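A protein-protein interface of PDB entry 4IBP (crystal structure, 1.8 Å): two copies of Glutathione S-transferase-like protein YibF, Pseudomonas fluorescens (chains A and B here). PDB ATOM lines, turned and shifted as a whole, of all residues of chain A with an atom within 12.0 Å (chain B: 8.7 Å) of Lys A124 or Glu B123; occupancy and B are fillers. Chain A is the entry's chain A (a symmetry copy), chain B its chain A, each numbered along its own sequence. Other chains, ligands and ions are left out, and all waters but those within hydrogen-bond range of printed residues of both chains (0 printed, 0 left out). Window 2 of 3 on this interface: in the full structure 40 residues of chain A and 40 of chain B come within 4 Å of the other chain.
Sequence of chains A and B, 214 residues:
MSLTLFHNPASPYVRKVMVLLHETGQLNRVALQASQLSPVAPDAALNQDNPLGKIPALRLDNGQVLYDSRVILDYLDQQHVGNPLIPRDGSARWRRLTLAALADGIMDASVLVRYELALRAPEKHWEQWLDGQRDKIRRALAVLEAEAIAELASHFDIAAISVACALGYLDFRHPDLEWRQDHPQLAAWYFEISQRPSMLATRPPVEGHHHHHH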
ATOM      1  N   VAL A  40      18.626  35.406 -33.865  1.00  0.00           N
ATOM      2  CA  VAL A  40      18.033  36.603 -33.266  1.00  0.00           C
ATOM      3  C   VAL A  40      19.000  37.786 -33.286  1.00  0.00           C
ATOM      4  O   VAL A  40      18.759  38.806 -32.639  1.00  0.00           O
ATOM      5  CB  VAL A  40      17.571  36.343 -31.815  1.00  0.00           C
ATOM      6  CG1 VAL A  40      16.580  35.194 -31.771  1.00  0.00           C
ATOM      7  CG2 VAL A  40      18.765  36.035 -30.921  1.00  0.00           C
ATOM      8  N   LEU A 112      20.680  23.496 -32.583  1.00  0.00           N
ATOM      9  CA  LEU A 112      19.354  23.865 -32.052  1.00  0.00           C
ATOM     10  C   LEU A 112      19.334  23.874 -30.523  1.00  0.00           C
ATOM     11  O   LEU A 112      18.756  24.767 -29.902  1.00  0.00           O
ATOM     12  CB  LEU A 112      18.248  22.938 -32.564  1.00  0.00           C
ATOM     13  CG  LEU A 112      17.635  23.168 -33.943  1.00  0.00           C
ATOM     14  CD1 LEU A 112      16.488  22.192 -34.164  1.00  0.00           C
ATOM     15  CD2 LEU A 112      17.161  24.593 -34.112  1.00  0.00           C
ATOM     16  N   VAL A 113      19.960  22.865 -29.927  1.00  0.00           N
ATOM     17  CA  VAL A 113      20.100  22.786 -28.476  1.00  0.00           C
ATOM     18  C   VAL A 113      20.905  23.968 -27.929  1.00  0.00           C
ATOM     19  O   VAL A 113      20.509  24.596 -26.946  1.00  0.00           O
ATOM     20  CB  VAL A 113      20.744  21.462 -28.064  1.00  0.00           C
ATOM     21  CG1 VAL A 113      21.276  21.528 -26.637  1.00  0.00           C
ATOM     22  CG2 VAL A 113      19.741  20.332 -28.210  1.00  0.00           C
ATOM     23  N   ARG A 114      22.021  24.271 -28.587  1.00  0.00           N
ATOM     24  CA  ARG A 114      22.895  25.378 -28.195  1.00  0.00           C
ATOM     25  C   ARG A 114      22.169  26.729 -28.179  1.00  0.00           C
ATOM     26  O   ARG A 114      22.332  27.511 -27.247  1.00  0.00           O
ATOM     27  CB  ARG A 114      24.117  25.435 -29.119  1.00  0.00           C
ATOM     28  CG  ARG A 114      24.912  26.733 -29.062  1.00  0.00           C
ATOM     29  CD  ARG A 114      25.669  26.869 -27.762  1.00  0.00           C
ATOM     30  NE  ARG A 114      26.371  28.146 -27.675  1.00  0.00           N
ATOM     31  CZ  ARG A 114      27.018  28.566 -26.591  1.00  0.00           C
ATOM     32  NH1 ARG A 114      27.045  27.809 -25.507  1.00  0.00           N
ATOM     33  NH2 ARG A 114      27.631  29.743 -26.593  1.00  0.00           N
ATOM     34  N   TYR A 115      21.369  26.995 -29.207  1.00  0.00           N
ATOM     35  CA  TYR A 115      20.606  28.246 -29.293  1.00  0.00           C
ATOM     36  C   TYR A 115      19.563  28.338 -28.187  1.00  0.00           C
ATOM     37  O   TYR A 115      19.321  29.409 -27.630  1.00  0.00           O
ATOM     38  CB  TYR A 115      19.911  28.367 -30.655  1.00  0.00           C
ATOM     39  CG  TYR A 115      20.845  28.696 -31.794  1.00  0.00           C
ATOM     40  CD1 TYR A 115      22.086  29.263 -31.548  1.00  0.00           C
ATOM     41  CD2 TYR A 115      20.491  28.432 -33.113  1.00  0.00           C
ATOM     42  CE1 TYR A 115      22.945  29.563 -32.570  1.00  0.00           C
ATOM     43  CE2 TYR A 115      21.350  28.733 -34.149  1.00  0.00           C
ATOM     44  CZ  TYR A 115      22.574  29.300 -33.868  1.00  0.00           C
ATOM     45  OH  TYR A 115      23.450  29.610 -34.877  1.00  0.00           O
ATOM     46  N   GLU A 116      18.946  27.202 -27.889  1.00  0.00           N
ATOM     47  CA  GLU A 116      17.894  27.118 -26.886  1.00  0.00           C
ATOM     48  C   GLU A 116      18.447  27.430 -25.497  1.00  0.00           C
ATOM     49  O   GLU A 116      17.890  28.247 -24.762  1.00  0.00           O
ATOM     50  CB  GLU A 116      17.291  25.714 -26.901  1.00  0.00           C
ATOM     51  CG  GLU A 116      16.212  25.470 -25.857  1.00  0.00           C
ATOM     52  CD  GLU A 116      14.827  25.836 -26.348  1.00  0.00           C
ATOM     53  OE1 GLU A 116      14.725  26.691 -27.253  1.00  0.00           O
ATOM     54  OE2 GLU A 116      13.845  25.261 -25.833  1.00  0.00           O
ATOM     55  N   LEU A 117      19.558  26.780 -25.160  1.00  0.00           N
ATOM     56  CA  LEU A 117      20.153  26.856 -23.830  1.00  0.00           C
ATOM     57  C   LEU A 117      20.935  28.142 -23.583  1.00  0.00           C
ATOM     58  O   LEU A 117      21.106  28.560 -22.440  1.00  0.00           O
ATOM     59  CB  LEU A 117      21.070  25.656 -23.591  1.00  0.00           C
ATOM     60  CG  LEU A 117      20.413  24.287 -23.490  1.00  0.00           C
ATOM     61  CD1 LEU A 117      21.445  23.195 -23.228  1.00  0.00           C
ATOM     62  CD2 LEU A 117      19.360  24.293 -22.401  1.00  0.00           C
ATOM     63  N   ALA A 118      21.421  28.761 -24.651  1.00  0.00           N
ATOM     64  CA  ALA A 118      22.309  29.910 -24.509  1.00  0.00           C
ATOM     65  C   ALA A 118      21.635  31.238 -24.827  1.00  0.00           C
ATOM     66  O   ALA A 118      22.100  32.288 -24.390  1.00  0.00           O
ATOM     67  CB  ALA A 118      23.548  29.733 -25.366  1.00  0.00           C
ATOM     68  N   LEU A 119      20.553  31.200 -25.597  1.00  0.00           N
ATOM     69  CA  LEU A 119      19.934  32.437 -26.066  1.00  0.00           C
ATOM     70  C   LEU A 119      18.483  32.610 -25.623  1.00  0.00           C
ATOM     71  O   LEU A 119      17.976  33.730 -25.588  1.00  0.00           O
ATOM     72  CB  LEU A 119      20.041  32.546 -27.590  1.00  0.00           C
ATOM     73  CG  LEU A 119      21.454  32.451 -28.159  1.00  0.00           C
ATOM     74  CD1 LEU A 119      21.430  32.517 -29.674  1.00  0.00           C
ATOM     75  CD2 LEU A 119      22.320  33.555 -27.586  1.00  0.00           C
ATOM     76  N   ARG A 120      17.818  31.509 -25.290  1.00  0.00           N
ATOM     77  CA  ARG A 120      16.412  31.571 -24.898  1.00  0.00           C
ATOM     78  C   ARG A 120      16.251  31.606 -23.380  1.00  0.00           C
ATOM     79  O   ARG A 120      16.879  30.824 -22.663  1.00  0.00           O
ATOM     80  CB  ARG A 120      15.631  30.390 -25.483  1.00  0.00           C
ATOM     81  CG  ARG A 120      14.123  30.493 -25.315  1.00  0.00           C
ATOM     82  CD  ARG A 120      13.408  29.276 -25.898  1.00  0.00           C
ATOM     83  NE  ARG A 120      13.279  29.329 -27.354  1.00  0.00           N
ATOM     84  CZ  ARG A 120      12.123  29.255 -28.008  1.00  0.00           C
ATOM     85  NH1 ARG A 120      10.984  29.121 -27.342  1.00  0.00           N
ATOM     86  NH2 ARG A 120      12.103  29.312 -29.332  1.00  0.00           N
ATOM     87  N   ALA A 121      15.407  32.521 -22.906  1.00  0.00           N
ATOM     88  CA  ALA A 121      15.138  32.680 -21.478  1.00  0.00           C
ATOM     89  C   ALA A 121      14.773  31.350 -20.822  1.00  0.00           C
ATOM     90  O   ALA A 121      13.777  30.727 -21.192  1.00  0.00           O
ATOM     91  CB  ALA A 121      14.037  33.700 -21.262  1.00  0.00           C
ATOM     92  N   PRO A 122      15.583  30.925 -19.834  1.00  0.00           N
ATOM     93  CA  PRO A 122      15.544  29.620 -19.153  1.00  0.00           C
ATOM     94  C   PRO A 122      14.154  29.233 -18.660  1.00  0.00           C
ATOM     95  O   PRO A 122      13.867  28.049 -18.469  1.00  0.00           O
ATOM     96  CB  PRO A 122      16.475  29.829 -17.957  1.00  0.00           C
ATOM     97  CG  PRO A 122      17.429  30.876 -18.407  1.00  0.00           C
ATOM     98  CD  PRO A 122      16.633  31.800 -19.280  1.00  0.00           C
ATOM     99  N   GLU A 123      13.305  30.232 -18.445  1.00  0.00           N
ATOM    100  CA  GLU A 123      11.929  29.989 -18.046  1.00  0.00           C
ATOM    101  C   GLU A 123      11.112  29.480 -19.239  1.00  0.00           C
ATOM    102  O   GLU A 123      10.024  28.925 -19.067  1.00  0.00           O
ATOM    103  CB  GLU A 123      11.307  31.268 -17.477  1.00  0.00           C
ATOM    104  CG  GLU A 123      10.696  32.194 -18.529  1.00  0.00           C
ATOM    105  CD  GLU A 123      11.465  33.493 -18.704  1.00  0.00           C
ATOM    106  OE1 GLU A 123      12.576  33.618 -18.140  1.00  0.00           O
ATOM    107  OE2 GLU A 123      10.951  34.391 -19.409  1.00  0.00           O
ATOM    108  N   LYS A 124      11.648  29.665 -20.446  1.00  0.00           N
ATOM    109  CA  LYS A 124      10.955  29.275 -21.673  1.00  0.00           C
ATOM    110  C   LYS A 124      11.545  28.023 -22.321  1.00  0.00           C
ATOM    111  O   LYS A 124      11.060  27.569 -23.360  1.00  0.00           O
ATOM    112  CB  LYS A 124      10.943  30.427 -22.672  1.00  0.00           C
ATOM    113  CG  LYS A 124       9.885  31.466 -22.392  1.00  0.00           C
ATOM    114  CD  LYS A 124      10.039  32.654 -23.317  1.00  0.00           C
ATOM    115  CE  LYS A 124       8.876  33.613 -23.173  1.00  0.00           C
ATOM    116  NZ  LYS A 124       9.064  34.796 -24.051  1.00  0.00           N
ATOM    117  N   HIS A 125      12.593  27.477 -21.710  1.00  0.00           N
ATOM    118  CA  HIS A 125      13.166  26.211 -22.152  1.00  0.00           C
ATOM    119  C   HIS A 125      12.096  25.125 -22.182  1.00  0.00           C
ATOM    120  O   HIS A 125      11.216  25.093 -21.323  1.00  0.00           O
ATOM    121  CB  HIS A 125      14.296  25.773 -21.216  1.00  0.00           C
ATOM    122  CG  HIS A 125      15.540  26.592 -21.340  1.00  0.00           C
ATOM    123  ND1 HIS A 125      16.715  26.259 -20.694  1.00  0.00           N
ATOM    124  CD2 HIS A 125      15.803  27.725 -22.030  1.00  0.00           C
ATOM    125  CE1 HIS A 125      17.641  27.152 -20.983  1.00  0.00           C
ATOM    126  NE2 HIS A 125      17.113  28.057 -21.791  1.00  0.00           N
ATOM    127  N   TRP A 126      12.172  24.240 -23.171  1.00  0.00           N
ATOM    128  CA  TRP A 126      11.266  23.100 -23.253  1.00  0.00           C
ATOM    129  C   TRP A 126      12.105  21.832 -23.182  1.00  0.00           C
ATOM    130  O   TRP A 126      12.893  21.553 -24.085  1.00  0.00           O
ATOM    131  CB  TRP A 126      10.464  23.159 -24.551  1.00  0.00           C
ATOM    132  CG  TRP A 126       9.468  22.053 -24.717  1.00  0.00           C
ATOM    133  CD1 TRP A 126       9.072  21.142 -23.776  1.00  0.00           C
ATOM    134  CD2 TRP A 126       8.740  21.739 -25.911  1.00  0.00           C
ATOM    135  NE1 TRP A 126       8.146  20.286 -24.316  1.00  0.00           N
ATOM    136  CE2 TRP A 126       7.923  20.631 -25.621  1.00  0.00           C
ATOM    137  CE3 TRP A 126       8.703  22.291 -27.194  1.00  0.00           C
ATOM    138  CZ2 TRP A 126       7.074  20.063 -26.577  1.00  0.00           C
ATOM    139  CZ3 TRP A 126       7.863  21.730 -28.136  1.00  0.00           C
ATOM    140  CH2 TRP A 126       7.061  20.626 -27.825  1.00  0.00           C
ATOM    141  N   GLU A 127      11.947  21.073 -22.103  1.00  0.00           N
ATOM    142  CA  GLU A 127      12.865  19.974 -21.813  1.00  0.00           C
ATOM    143  C   GLU A 127      12.661  18.764 -22.722  1.00  0.00           C
ATOM    144  O   GLU A 127      13.610  18.046 -23.042  1.00  0.00           O
ATOM    145  CB  GLU A 127      12.753  19.558 -20.339  1.00  0.00           C
ATOM    146  CG  GLU A 127      13.938  18.746 -19.823  1.00  0.00           C
ATOM    147  CD  GLU A 127      15.230  19.542 -19.823  1.00  0.00           C
ATOM    148  OE1 GLU A 127      15.155  20.789 -19.800  1.00  0.00           O
ATOM    149  OE2 GLU A 127      16.316  18.921 -19.847  1.00  0.00           O
ATOM    150  N   GLN A 128      11.420  18.538 -23.132  1.00  0.00           N
ATOM    151  CA  GLN A 128      11.117  17.405 -23.990  1.00  0.00           C
ATOM    152  C   GLN A 128      11.631  17.678 -25.406  1.00  0.00           C
ATOM    153  O   GLN A 128      11.900  16.754 -26.175  1.00  0.00           O
ATOM    154  CB  GLN A 128       9.612  17.143 -24.000  1.00  0.00           C
ATOM    155  CG  GLN A 128       9.215  15.743 -24.445  1.00  0.00           C
ATOM    156  CD  GLN A 128       7.714  15.588 -24.563  1.00  0.00           C
ATOM    157  OE1 GLN A 128       6.965  16.550 -24.384  1.00  0.00           O
ATOM    158  NE2 GLN A 128       7.264  14.377 -24.872  1.00  0.00           N
ATOM    159  N   TRP A 129      11.770  18.958 -25.735  1.00  0.00           N
ATOM    160  CA  TRP A 129      12.307  19.376 -27.020  1.00  0.00           C
ATOM    161  C   TRP A 129      13.815  19.154 -27.063  1.00  0.00           C
ATOM    162  O   TRP A 129      14.322  18.467 -27.946  1.00  0.00           O
ATOM    163  CB  TRP A 129      11.981  20.843 -27.252  1.00  0.00           C
ATOM    164  CG  TRP A 129      12.611  21.436 -28.479  1.00  0.00           C
ATOM    165  CD1 TRP A 129      13.781  22.142 -28.544  1.00  0.00           C
ATOM    166  CD2 TRP A 129      12.094  21.394 -29.815  1.00  0.00           C
ATOM    167  NE1 TRP A 129      14.023  22.535 -29.838  1.00  0.00           N
ATOM    168  CE2 TRP A 129      13.004  22.092 -30.637  1.00  0.00           C
ATOM    169  CE3 TRP A 129      10.954  20.834 -30.393  1.00  0.00           C
ATOM    170  CZ2 TRP A 129      12.802  22.239 -32.016  1.00  0.00           C
ATOM    171  CZ3 TRP A 129      10.756  20.981 -31.756  1.00  0.00           C
ATOM    172  CH2 TRP A 129      11.676  21.676 -32.553  1.00  0.00           C
ATOM    173  N   LEU A 130      14.524  19.738 -26.099  1.00  0.00           N
ATOM    174  CA  LEU A 130      15.972  19.572 -25.976  1.00  0.00           C
ATOM    175  C   LEU A 130      16.355  18.095 -25.943  1.00  0.00           C
ATOM    176  O   LEU A 130      17.323  17.678 -26.585  1.00  0.00           O
ATOM    177  CB  LEU A 130      16.489  20.275 -24.718  1.00  0.00           C
ATOM    178  CG  LEU A 130      16.572  21.798 -24.745  1.00  0.00           C
ATOM    179  CD1 LEU A 130      16.485  22.371 -23.342  1.00  0.00           C
ATOM    180  CD2 LEU A 130      17.860  22.250 -25.407  1.00  0.00           C
ATOM    181  N   ASP A 131      15.585  17.313 -25.193  1.00  0.00           N
ATOM    182  CA  ASP A 131      15.819  15.880 -25.074  1.00  0.00           C
ATOM    183  C   ASP A 131      15.568  15.162 -26.394  1.00  0.00           C
ATOM    184  O   ASP A 131      16.237  14.174 -26.710  1.00  0.00           O
ATOM    185  CB  ASP A 131      14.934  15.285 -23.976  1.00  0.00           C
ATOM    186  CG  ASP A 131      15.477  15.547 -22.581  1.00  0.00           C
ATOM    187  OD1 ASP A 131      16.719  15.552 -22.419  1.00  0.00           O
ATOM    188  OD2 ASP A 131      14.664  15.745 -21.651  1.00  0.00           O
ATOM    189  N   GLU B 116       7.149  25.273 -33.120  1.00  0.00           N
ATOM    190  CA  GLU B 116       7.121  26.200 -31.999  1.00  0.00           C
ATOM    191  C   GLU B 116       5.684  26.580 -31.648  1.00  0.00           C
ATOM    192  O   GLU B 116       5.277  26.516 -30.487  1.00  0.00           O
ATOM    193  CB  GLU B 116       7.916  27.456 -32.360  1.00  0.00           C
ATOM    194  CG  GLU B 116       7.921  28.539 -31.292  1.00  0.00           C
ATOM    195  CD  GLU B 116       9.048  28.373 -30.295  1.00  0.00           C
ATOM    196  OE1 GLU B 116       9.519  27.231 -30.114  1.00  0.00           O
ATOM    197  OE2 GLU B 116       9.466  29.389 -29.700  1.00  0.00           O
ATOM    198  N   ARG B 120       4.771  23.705 -28.823  1.00  0.00           N
ATOM    199  CA  ARG B 120       5.365  24.279 -27.617  1.00  0.00           C
ATOM    200  C   ARG B 120       4.367  25.148 -26.856  1.00  0.00           C
ATOM    201  O   ARG B 120       3.677  25.980 -27.451  1.00  0.00           O
ATOM    202  CB  ARG B 120       6.617  25.090 -27.960  1.00  0.00           C
ATOM    203  CG  ARG B 120       7.425  25.536 -26.750  1.00  0.00           C
ATOM    204  CD  ARG B 120       8.645  26.358 -27.160  1.00  0.00           C
ATOM    205  NE  ARG B 120       9.757  25.536 -27.638  1.00  0.00           N
ATOM    206  CZ  ARG B 120      10.982  25.557 -27.119  1.00  0.00           C
ATOM    207  NH1 ARG B 120      11.265  26.359 -26.102  1.00  0.00           N
ATOM    208  NH2 ARG B 120      11.929  24.775 -27.618  1.00  0.00           N
ATOM    209  N   ALA B 121       4.302  24.945 -25.541  1.00  0.00           N
ATOM    210  CA  ALA B 121       3.402  25.699 -24.671  1.00  0.00           C
ATOM    211  C   ALA B 121       3.542  27.205 -24.884  1.00  0.00           C
ATOM    212  O   ALA B 121       4.618  27.766 -24.672  1.00  0.00           O
ATOM    213  CB  ALA B 121       3.655  25.342 -23.219  1.00  0.00           C
ATOM    214  N   PRO B 122       2.440  27.859 -25.298  1.00  0.00           N
ATOM    215  CA  PRO B 122       2.348  29.265 -25.721  1.00  0.00           C
ATOM    216  C   PRO B 122       2.987  30.239 -24.737  1.00  0.00           C
ATOM    217  O   PRO B 122       3.370  31.348 -25.117  1.00  0.00           O
ATOM    218  CB  PRO B 122       0.838  29.509 -25.780  1.00  0.00           C
ATOM    219  CG  PRO B 122       0.257  28.171 -26.063  1.00  0.00           C
ATOM    220  CD  PRO B 122       1.125  27.190 -25.333  1.00  0.00           C
ATOM    221  N   GLU B 123       3.086  29.826 -23.479  1.00  0.00           N
ATOM    222  CA  GLU B 123       3.743  30.631 -22.464  1.00  0.00           C
ATOM    223  C   GLU B 123       5.264  30.591 -22.654  1.00  0.00           C
ATOM    224  O   GLU B 123       5.990  31.428 -22.113  1.00  0.00           O
ATOM    225  CB  GLU B 123       3.365  30.134 -21.064  1.00  0.00           C
ATOM    226  CG  GLU B 123       4.244  28.999 -20.540  1.00  0.00           C
ATOM    227  CD  GLU B 123       3.511  27.672 -20.435  1.00  0.00           C
ATOM    228  OE1 GLU B 123       2.364  27.574 -20.930  1.00  0.00           O
ATOM    229  OE2 GLU B 123       4.087  26.725 -19.853  1.00  0.00           O
ATOM    230  N   LYS B 124       5.737  29.617 -23.432  1.00  0.00           N
ATOM    231  CA  LYS B 124       7.170  29.430 -23.659  1.00  0.00           C
ATOM    232  C   LYS B 124       7.617  29.870 -25.052  1.00  0.00           C
ATOM    233  O   LYS B 124       8.800  29.778 -25.386  1.00  0.00           O
ATOM    234  CB  LYS B 124       7.566  27.976 -23.415  1.00  0.00           C
ATOM    235  CG  LYS B 124       7.740  27.628 -21.958  1.00  0.00           C
ATOM    236  CD  LYS B 124       7.967  26.143 -21.783  1.00  0.00           C
ATOM    237  CE  LYS B 124       8.329  25.810 -20.350  1.00  0.00           C
ATOM    238  NZ  LYS B 124       8.502  24.344 -20.183  1.00  0.00           N
ATOM    239  N   HIS B 125       6.669  30.338 -25.858  1.00  0.00           N
ATOM    240  CA  HIS B 125       6.983  30.910 -27.162  1.00  0.00           C
ATOM    241  C   HIS B 125       7.994  32.043 -27.016  1.00  0.00           C
ATOM    242  O   HIS B 125       7.946  32.800 -26.048  1.00  0.00           O
ATOM    243  CB  HIS B 125       5.719  31.453 -27.834  1.00  0.00           C
ATOM    244  CG  HIS B 125       4.784  30.393 -28.319  1.00  0.00           C
ATOM    245  ND1 HIS B 125       3.670  30.679 -29.084  1.00  0.00           N
ATOM    246  CD2 HIS B 125       4.789  29.050 -28.156  1.00  0.00           C
ATOM    247  CE1 HIS B 125       3.034  29.559 -29.366  1.00  0.00           C
ATOM    248  NE2 HIS B 125       3.692  28.553 -28.812  1.00  0.00           N
ATOM    249  N   TRP B 126       8.908  32.154 -27.975  1.00  0.00           N
ATOM    250  CA  TRP B 126       9.868  33.252 -27.997  1.00  0.00           C
ATOM    251  C   TRP B 126       9.646  34.038 -29.282  1.00  0.00           C
ATOM    252  O   TRP B 126       9.873  33.523 -30.377  1.00  0.00           O
ATOM    253  CB  TRP B 126      11.292  32.707 -27.924  1.00  0.00           C
ATOM    254  CG  TRP B 126      12.360  33.758 -27.898  1.00  0.00           C
ATOM    255  CD1 TRP B 126      12.195  35.105 -27.737  1.00  0.00           C
ATOM    256  CD2 TRP B 126      13.768  33.539 -28.043  1.00  0.00           C
ATOM    257  NE1 TRP B 126      13.415  35.734 -27.775  1.00  0.00           N
ATOM    258  CE2 TRP B 126      14.395  34.796 -27.960  1.00  0.00           C
ATOM    259  CE3 TRP B 126      14.555  32.400 -28.236  1.00  0.00           C
ATOM    260  CZ2 TRP B 126      15.782  34.943 -28.061  1.00  0.00           C
ATOM    261  CZ3 TRP B 126      15.925  32.547 -28.335  1.00  0.00           C
ATOM    262  CH2 TRP B 126      16.526  33.809 -28.251  1.00  0.00           C
ATOM    263  N   GLU B 127       9.188  35.278 -29.151  1.00  0.00           N
ATOM    264  CA  GLU B 127       8.710  36.033 -30.306  1.00  0.00           C
ATOM    265  C   GLU B 127       9.837  36.521 -31.214  1.00  0.00           C
ATOM    266  O   GLU B 127       9.670  36.629 -32.430  1.00  0.00           O
ATOM    267  CB  GLU B 127       7.842  37.215 -29.852  1.00  0.00           C
ATOM    268  CG  GLU B 127       6.951  37.797 -30.946  1.00  0.00           C
ATOM    269  CD  GLU B 127       5.904  36.811 -31.427  1.00  0.00           C
ATOM    270  OE1 GLU B 127       5.579  35.876 -30.663  1.00  0.00           O
ATOM    271  OE2 GLU B 127       5.408  36.970 -32.565  1.00  0.00           O
ATOM    272  N   GLN B 128      10.985  36.820 -30.618  1.00  0.00           N
ATOM    273  CA  GLN B 128      12.117  37.306 -31.390  1.00  0.00           C
ATOM    274  C   GLN B 128      12.729  36.153 -32.190  1.00  0.00           C
ATOM    275  O   GLN B 128      13.373  36.363 -33.217  1.00  0.00           O
ATOM    276  CB  GLN B 128      13.154  37.933 -30.461  1.00  0.00           C
ATOM    277  CG  GLN B 128      14.124  38.885 -31.145  1.00  0.00           C
ATOM    278  CD  GLN B 128      15.207  39.367 -30.203  1.00  0.00           C
ATOM    279  OE1 GLN B 128      15.279  38.934 -29.051  1.00  0.00           O
ATOM    280  NE2 GLN B 128      16.060  40.263 -30.686  1.00  0.00           N
ATOM    281  N   TRP B 129      12.511  34.934 -31.706  1.00  0.00           N
ATOM    282  CA  TRP B 129      12.973  33.735 -32.387  1.00  0.00           C
ATOM    283  C   TRP B 129      12.110  33.453 -33.612  1.00  0.00           C
ATOM    284  O   TRP B 129      12.618  33.347 -34.725  1.00  0.00           O
ATOM    285  CB  TRP B 129      12.929  32.557 -31.425  1.00  0.00           C
ATOM    286  CG  TRP B 129      13.241  31.229 -32.051  1.00  0.00           C
ATOM    287  CD1 TRP B 129      12.343  30.310 -32.520  1.00  0.00           C
ATOM    288  CD2 TRP B 129      14.540  30.660 -32.254  1.00  0.00           C
ATOM    289  NE1 TRP B 129      13.006  29.209 -33.007  1.00  0.00           N
ATOM    290  CE2 TRP B 129      14.353  29.398 -32.854  1.00  0.00           C
ATOM    291  CE3 TRP B 129      15.838  31.095 -31.987  1.00  0.00           C
ATOM    292  CZ2 TRP B 129      15.429  28.566 -33.194  1.00  0.00           C
ATOM    293  CZ3 TRP B 129      16.900  30.272 -32.324  1.00  0.00           C
ATOM    294  CH2 TRP B 129      16.690  29.023 -32.923  1.00  0.00           C
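OE2 of Glu B116 lies within salt-bridge range of NH2 of Arg A120 (2.7 Å). NH2 of Arg B120 is in salt-bridge range of OE2 of Glu A116 (2.7 Å). O of Lys A124 sits at hydrogen-bond distance from NH1 of Arg B120, at 3.0 Å. O of Lys B124 is in hydrogen-bond range of NH1 of Arg A120, at 3.0 Å. The side-chain amino group of Lys B124 sits at hydrogen-bond distance from the backbone carbonyl oxygen of His A125, at 3.0 Å. O of His B125 is in hydrogen-bond range of NZ of Lys A124 (3.0 Å). The guanidinium group (NH1) of Arg A120 lies close to the guanidinium group (NH1) of Arg B120, at 3.0 Å.
NE of Arg B120 is in salt-bridge range of OE1 of Glu B116 (3.0 Å). NE2 of His B125 sits at hydrogen-bond distance from O of Glu B116, at 3.1 Å. The backbone NH (N) of Trp B126 lies within hydrogen-bond range of the side-chain carboxylate (OE2) of Glu B116, 3.3 Å away. The backbone carbonyl oxygen of Arg B120 lies within hydrogen-bond range of a ring nitrogen (NE2) of His B125. O of Tyr A115 lies within hydrogen-bond range of N of Arg A120 (3.5 Å).
Trp B126 touches Val A40. O of Val A40 touches NE2 of Gln B128, 3.6 Å away. Val A40 touches Trp B129. Tyr A115 touches Trp B129 (CD2 to CH2, 3.9 Å). Trp B126 touches Leu A119 (CH2 to O, 3.0 Å). CD1 of Trp B129 touches NH2 of Arg A120, 3.3 Å away. CE of Lys B124 touches O of Glu A123, 3.8 Å away. Glu B123 touches Lys A124 (O to CE, 3.8 Å). Lys A124 touches Lys B124. Arg B120 touches Trp A126 (NE to CE3, 3.4 Å).
Of the printed residues of chain A, Glu B123 touches Lys A124. No residue of chain A comes within 4 Å of Ala B121. No residue of chain A comes within 4 Å of Pro B122. Lys B124 touches just these residues of chain A: Arg A120 (3.0 Å), Glu A123 (3.8 Å), Lys A124 (3.5 Å) and His A125 (3.0 Å). His B125 touches just one residue of chain A: Lys A124. Of the printed residues of chain B, Trp A129 touches Arg B120 (3.3 Å). Of the printed residues of chain A, Glu B116 touches Arg A120 (2.7 Å). Printed residues of chain B within 4 Å of Val A40: Trp B126 (3.8 Å), Gln B128 (3.6 Å) and Trp B129 (3.9 Å). Of the printed residues of chain B, His A125 touches Lys B124 (3.0 Å). Val A113 touches none of the printed residues of chain B. The nearest residue of chain B that does not touch Lys A124 is Trp B126 (4.3 Å). The nearest residue of chain A that does not touch Glu B123 is Glu A123 (5.6 Å). The nearest printed residue of chain B that does not touch Trp A126 is Lys B124 (4.3 Å).
Printed residues of chain B that touch a printed residue of chain A: Glu B116, Arg B120, Glu B123, Lys B124, His B125, Trp B126, Gln B128 and Trp B129. Along chain B the printed residues that touch a printed residue of chain A span positions 116 to 129. Of the 21 printed residues of chain A, 10 touch a printed residue of chain B. Printed residues of chain A that touch a printed residue of chain B: Val A40, Tyr A115, Glu A116, Leu A119, Arg A120, Glu A123, Lys A124, His A125, Trp A126 and Trp A129. Hydrophobic or aromatic side chains of chain A that line the printed part of chain B: Val A40, Tyr A115, Leu A119, Trp A126 and Trp A129. Among the printed residues, Asp or Glu carboxylates within 4 Å of a Lys or Arg side-chain nitrogen of the other chain: Glu A116 with Arg B120 (2.7 Å) and Arg A120 with Glu B116 (2.7 Å).
Glu A116 touches Arg B120, and with the chains exchanged Arg A120 touches Glu B116. Glu A123 touches Lys B124, and with the chains exchanged Lys A124 touches Glu B123. Lys B124 touches its own counterpart, Lys A124. Lys A124 touches His B125, and with the chains exchanged His A125 touches Lys B124. Positions printed for both chains: 116, 120, 121, 122, 123, 124, 125, 126, 127, 128 and 129.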
